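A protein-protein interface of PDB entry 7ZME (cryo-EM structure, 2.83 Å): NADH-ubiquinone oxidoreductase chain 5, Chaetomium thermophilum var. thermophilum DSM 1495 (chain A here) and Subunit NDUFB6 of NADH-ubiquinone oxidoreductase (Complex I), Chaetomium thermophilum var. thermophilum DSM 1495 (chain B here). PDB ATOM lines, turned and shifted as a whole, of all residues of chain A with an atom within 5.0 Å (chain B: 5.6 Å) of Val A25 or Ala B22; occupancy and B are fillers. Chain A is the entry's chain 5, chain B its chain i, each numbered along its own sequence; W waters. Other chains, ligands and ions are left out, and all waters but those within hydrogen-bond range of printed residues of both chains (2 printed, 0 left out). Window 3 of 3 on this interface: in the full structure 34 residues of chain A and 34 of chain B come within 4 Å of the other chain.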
ATOM      1  N   GLY A  20      13.896  25.245  27.233  1.00  0.00           N
ATOM      2  CA  GLY A  20      13.174  23.975  27.096  1.00  0.00           C
ATOM      3  C   GLY A  20      13.175  23.209  28.383  1.00  0.00           C
ATOM      4  O   GLY A  20      12.399  22.283  28.503  1.00  0.00           O
ATOM      5  N   VAL A  23       9.911  24.716  29.733  1.00  0.00           N
ATOM      6  CA  VAL A  23       8.624  24.487  29.037  1.00  0.00           C
ATOM      7  C   VAL A  23       8.396  23.001  28.898  1.00  0.00           C
ATOM      8  O   VAL A  23       7.264  22.616  28.567  1.00  0.00           O
ATOM      9  CB  VAL A  23       8.528  25.250  27.701  1.00  0.00           C
ATOM     10  CG1 VAL A  23       8.406  26.743  27.939  1.00  0.00           C
ATOM     11  CG2 VAL A  23       9.682  24.948  26.762  1.00  0.00           C
ATOM     12  N   GLY A  24       9.440  22.206  29.084  1.00  0.00           N
ATOM     13  CA  GLY A  24       9.282  20.780  28.900  1.00  0.00           C
ATOM     14  C   GLY A  24       9.187  20.372  27.443  1.00  0.00           C
ATOM     15  O   GLY A  24       9.517  21.118  26.524  1.00  0.00           O
ATOM     16  N   VAL A  25       8.725  19.140  27.243  1.00  0.00           N
ATOM     17  CA  VAL A  25       8.605  18.590  25.896  1.00  0.00           C
ATOM     18  C   VAL A  25       7.340  19.089  25.221  1.00  0.00           C
ATOM     19  O   VAL A  25       7.385  19.736  24.169  1.00  0.00           O
ATOM     20  CB  VAL A  25       8.646  17.053  25.939  1.00  0.00           C
ATOM     21  CG1 VAL A  25       8.802  16.495  24.542  1.00  0.00           C
ATOM     22  CG2 VAL A  25       9.770  16.575  26.845  1.00  0.00           C
ATOM     23  N   SER A  26       6.188  18.790  25.819  1.00  0.00           N
ATOM     24  CA  SER A  26       4.917  19.148  25.207  1.00  0.00           C
ATOM     25  C   SER A  26       4.707  20.656  25.173  1.00  0.00           C
ATOM     26  O   SER A  26       4.028  21.161  24.276  1.00  0.00           O
ATOM     27  CB  SER A  26       3.784  18.449  25.952  1.00  0.00           C
ATOM     28  OG  SER A  26       3.739  18.870  27.299  1.00  0.00           O
ATOM     29  N   GLY A  27       5.268  21.386  26.135  1.00  0.00           N
ATOM     30  CA  GLY A  27       5.220  22.835  26.062  1.00  0.00           C
ATOM     31  C   GLY A  27       6.051  23.387  24.921  1.00  0.00           C
ATOM     32  O   GLY A  27       5.624  24.306  24.218  1.00  0.00           O
ATOM     33  N   ALA A  28       7.252  22.836  24.725  1.00  0.00           N
ATOM     34  CA  ALA A  28       8.093  23.262  23.612  1.00  0.00           C
ATOM     35  C   ALA A  28       7.425  22.973  22.278  1.00  0.00           C
ATOM     36  O   ALA A  28       7.482  23.792  21.355  1.00  0.00           O
ATOM     37  CB  ALA A  28       9.455  22.576  23.693  1.00  0.00           C
ATOM     38  N   GLN A  29       6.791  21.805  22.156  1.00  0.00           N
ATOM     39  CA  GLN A  29       6.044  21.492  20.945  1.00  0.00           C
ATOM     40  C   GLN A  29       4.855  22.425  20.775  1.00  0.00           C
ATOM     41  O   GLN A  29       4.574  22.890  19.667  1.00  0.00           O
ATOM     42  CB  GLN A  29       5.586  20.034  20.979  1.00  0.00           C
ATOM     43  CG  GLN A  29       6.720  19.038  20.920  1.00  0.00           C
ATOM     44  CD  GLN A  29       6.319  17.669  21.404  1.00  0.00           C
ATOM     45  OE1 GLN A  29       5.369  17.525  22.168  1.00  0.00           O
ATOM     46  NE2 GLN A  29       7.042  16.650  20.965  1.00  0.00           N
ATOM     47  N   LEU A  30       4.147  22.714  21.866  1.00  0.00           N
ATOM     48  CA  LEU A  30       2.987  23.592  21.780  1.00  0.00           C
ATOM     49  C   LEU A  30       3.381  24.988  21.323  1.00  0.00           C
ATOM     50  O   LEU A  30       2.677  25.608  20.520  1.00  0.00           O
ATOM     51  CB  LEU A  30       2.277  23.656  23.129  1.00  0.00           C
ATOM     52  CG  LEU A  30       0.790  23.979  23.065  1.00  0.00           C
ATOM     53  CD1 LEU A  30       0.072  22.952  22.207  1.00  0.00           C
ATOM     54  CD2 LEU A  30       0.201  24.022  24.464  1.00  0.00           C
ATOM     55  N   ASN A 110      14.321  16.252  22.655  1.00  0.00           N
ATOM     56  CA  ASN A 110      13.194  16.611  21.820  1.00  0.00           C
ATOM     57  C   ASN A 110      12.931  18.114  21.834  1.00  0.00           C
ATOM     58  O   ASN A 110      12.264  18.623  20.930  1.00  0.00           O
ATOM     59  CB  ASN A 110      11.974  15.803  22.289  1.00  0.00           C
ATOM     60  CG  ASN A 110      10.788  15.908  21.359  1.00  0.00           C
ATOM     61  OD1 ASN A 110      10.822  16.600  20.353  1.00  0.00           O
ATOM     62  ND2 ASN A 110       9.733  15.179  21.681  1.00  0.00           N
ATOM     63  N   GLN A 111      13.468  18.849  22.813  1.00  0.00           N
ATOM     64  CA  GLN A 111      13.359  20.304  22.758  1.00  0.00           C
ATOM     65  C   GLN A 111      14.306  20.884  21.721  1.00  0.00           C
ATOM     66  O   GLN A 111      13.947  21.818  20.999  1.00  0.00           O
ATOM     67  CB  GLN A 111      13.669  20.949  24.108  1.00  0.00           C
ATOM     68  CG  GLN A 111      12.627  20.765  25.168  1.00  0.00           C
ATOM     69  CD  GLN A 111      12.574  19.348  25.643  1.00  0.00           C
ATOM     70  OE1 GLN A 111      11.563  18.685  25.524  1.00  0.00           O
ATOM     71  NE2 GLN A 111      13.666  18.886  26.231  1.00  0.00           N
ATOM     72  N   ALA B  17      18.275  23.391  26.953  1.00  0.00           N
ATOM     73  CA  ALA B  17      17.196  22.765  26.204  1.00  0.00           C
ATOM     74  C   ALA B  17      16.514  21.650  26.983  1.00  0.00           C
ATOM     75  O   ALA B  17      15.598  21.018  26.455  1.00  0.00           O
ATOM     76  CB  ALA B  17      17.724  22.233  24.872  1.00  0.00           C
ATOM     77  N   GLY B  18      16.940  21.389  28.213  1.00  0.00           N
ATOM     78  CA  GLY B  18      16.222  20.484  29.082  1.00  0.00           C
ATOM     79  C   GLY B  18      16.989  19.260  29.525  1.00  0.00           C
ATOM     80  O   GLY B  18      16.969  18.908  30.708  1.00  0.00           O
ATOM     81  N   GLY B  19      17.689  18.612  28.605  1.00  0.00           N
ATOM     82  CA  GLY B  19      18.375  17.389  28.957  1.00  0.00           C
ATOM     83  C   GLY B  19      17.925  16.209  28.129  1.00  0.00           C
ATOM     84  O   GLY B  19      17.923  16.279  26.899  1.00  0.00           O
ATOM     85  N   TRP B  20      17.541  15.111  28.779  1.00  0.00           N
ATOM     86  CA  TRP B  20      17.215  13.891  28.054  1.00  0.00           C
ATOM     87  C   TRP B  20      15.716  13.680  27.879  1.00  0.00           C
ATOM     88  O   TRP B  20      15.238  13.607  26.750  1.00  0.00           O
ATOM     89  CB  TRP B  20      17.868  12.683  28.728  1.00  0.00           C
ATOM     90  CG  TRP B  20      19.241  12.451  28.211  1.00  0.00           C
ATOM     91  CD1 TRP B  20      19.606  11.566  27.244  1.00  0.00           C
ATOM     92  CD2 TRP B  20      20.430  13.147  28.591  1.00  0.00           C
ATOM     93  NE1 TRP B  20      20.955  11.645  27.014  1.00  0.00           N
ATOM     94  CE2 TRP B  20      21.484  12.612  27.828  1.00  0.00           C
ATOM     95  CE3 TRP B  20      20.710  14.154  29.515  1.00  0.00           C
ATOM     96  CZ2 TRP B  20      22.792  13.050  27.961  1.00  0.00           C
ATOM     97  CZ3 TRP B  20      22.006  14.590  29.643  1.00  0.00           C
ATOM     98  CH2 TRP B  20      23.034  14.038  28.872  1.00  0.00           C
ATOM     99  N   TYR B  21      14.957  13.597  28.956  1.00  0.00           N
ATOM    100  CA  TYR B  21      13.514  13.464  28.802  1.00  0.00           C
ATOM    101  C   TYR B  21      12.812  14.502  29.647  1.00  0.00           C
ATOM    102  O   TYR B  21      11.814  14.226  30.315  1.00  0.00           O
ATOM    103  CB  TYR B  21      13.051  12.051  29.144  1.00  0.00           C
ATOM    104  CG  TYR B  21      13.584  11.001  28.196  1.00  0.00           C
ATOM    105  CD1 TYR B  21      14.843  10.447  28.379  1.00  0.00           C
ATOM    106  CD2 TYR B  21      12.835  10.574  27.110  1.00  0.00           C
ATOM    107  CE1 TYR B  21      15.337   9.499  27.512  1.00  0.00           C
ATOM    108  CE2 TYR B  21      13.321   9.623  26.239  1.00  0.00           C
ATOM    109  CZ  TYR B  21      14.571   9.088  26.446  1.00  0.00           C
ATOM    110  OH  TYR B  21      15.057   8.139  25.578  1.00  0.00           O
ATOM    111  N   ALA B  22      13.319  15.730  29.595  1.00  0.00           N
ATOM    112  CA  ALA B  22      13.010  16.745  30.592  1.00  0.00           C
ATOM    113  C   ALA B  22      11.616  17.314  30.364  1.00  0.00           C
ATOM    114  O   ALA B  22      11.354  17.960  29.346  1.00  0.00           O
ATOM    115  CB  ALA B  22      14.059  17.849  30.554  1.00  0.00           C
ATOM    116  N   GLN B  23      10.713  17.021  31.292  1.00  0.00           N
ATOM    117  CA  GLN B  23       9.404  17.688  31.293  1.00  0.00           C
ATOM    118  C   GLN B  23       9.254  18.124  32.742  1.00  0.00           C
ATOM    119  O   GLN B  23       9.300  17.266  33.620  1.00  0.00           O
ATOM    120  CB  GLN B  23       8.258  16.811  30.815  1.00  0.00           C
ATOM    121  CG  GLN B  23       6.921  17.536  30.833  1.00  0.00           C
ATOM    122  CD  GLN B  23       6.047  17.217  29.647  1.00  0.00           C
ATOM    123  OE1 GLN B  23       6.391  17.489  28.505  1.00  0.00           O
ATOM    124  NE2 GLN B  23       4.889  16.642  29.917  1.00  0.00           N
ATOM    125  N   PRO B  24       9.132  19.425  33.025  1.00  0.00           N
ATOM    126  CA  PRO B  24       8.936  19.876  34.372  1.00  0.00           C
ATOM    127  C   PRO B  24       7.523  19.535  34.870  1.00  0.00           C
ATOM    128  O   PRO B  24       6.673  19.208  34.073  1.00  0.00           O
ATOM    129  CB  PRO B  24       9.258  21.365  34.235  1.00  0.00           C
ATOM    130  CG  PRO B  24       8.799  21.707  32.872  1.00  0.00           C
ATOM    131  CD  PRO B  24       9.240  20.509  32.071  1.00  0.00           C
HETATM  132  O   HOH W   1      14.505  16.463  26.284  1.00  0.00           O
HETATM  133  O   HOH W   2      16.478  18.716  24.342  1.00  0.00           O
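Water W1 lies within hydrogen-bond range of NE2 of Gln A111, O of Trp B20 and O of Gly B19.
Water W2 lies within hydrogen-bond range of the backbone carbonyl oxygen (O) of Ala B17 (3.2 Å) and the backbone NH (N) of Gln A111 (3.4 Å).
Of the 11 printed residues of chain A, 5 touch a printed residue of chain B.
Printed residues of chain B that touch a printed residue of chain A: Ala B17, Ala B22, Gln B23 and Pro B24.
Among the printed residues, 9 pairs touch across the chains.
Among the printed residues, no Asp or Glu carboxylate lies within 4 Å of a Lys or Arg side-chain nitrogen of the other chain.
The backbone carbonyl oxygen of Ala B17 sits at hydrogen-bond distance from the side-chain amide nitrogen of Gln A111 (2.9 Å).
N of Val A25 is in hydrogen-bond range of OE1 of Gln B23, 3.1 Å away.
N of Ser A26 sits at hydrogen-bond distance from OE1 of Gln B23 (3.0 Å).
Of chain B, only Ala B22 (3.3 Å) and Gln B23 (3.1 Å) come within 4 Å of Val A25.
Printed residues of chain A within 4 Å of Ala B22: Gly A24, Val A25 and Gln A111.
Printed residues of chain A within 4 Å of Gln B23: Gly A24, Val A25 and Ser A26.
Of the printed residues of chain A, Ala B17 touches Gly A20 (3.8 Å) and Gln A111 (2.9 Å).
Gly B19 touches none of the printed residues of chain A.
The nearest residue of chain B that does not touch Val A25 is Tyr B21 (4.6 Å).
The nearest residue of chain A that does not touch Ala B22 is Gly A20 (4.5 Å).
Among the printed residues, merely in contact across the chains: Gly A24 with Pro B24 (3.2 Å), Val A25 with Ala B22 (3.3 Å), Gly A24 with Ala B22 (3.5 Å), Gly A20 with Ala B17 (3.8 Å), Gln A111 with Ala B22 (3.9 Å) and Gly A24 with Gln B23 (3.9 Å).
The backbone carbonyl oxygen (O) of Gly A24 sits close to the side-chain amide oxygen (OE1) of Gln A111, at 3.3 Å.
The side-chain amide oxygen (OE1) of Gln A111 sits close to the backbone NH (N) of Val A25 (3.3 Å).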
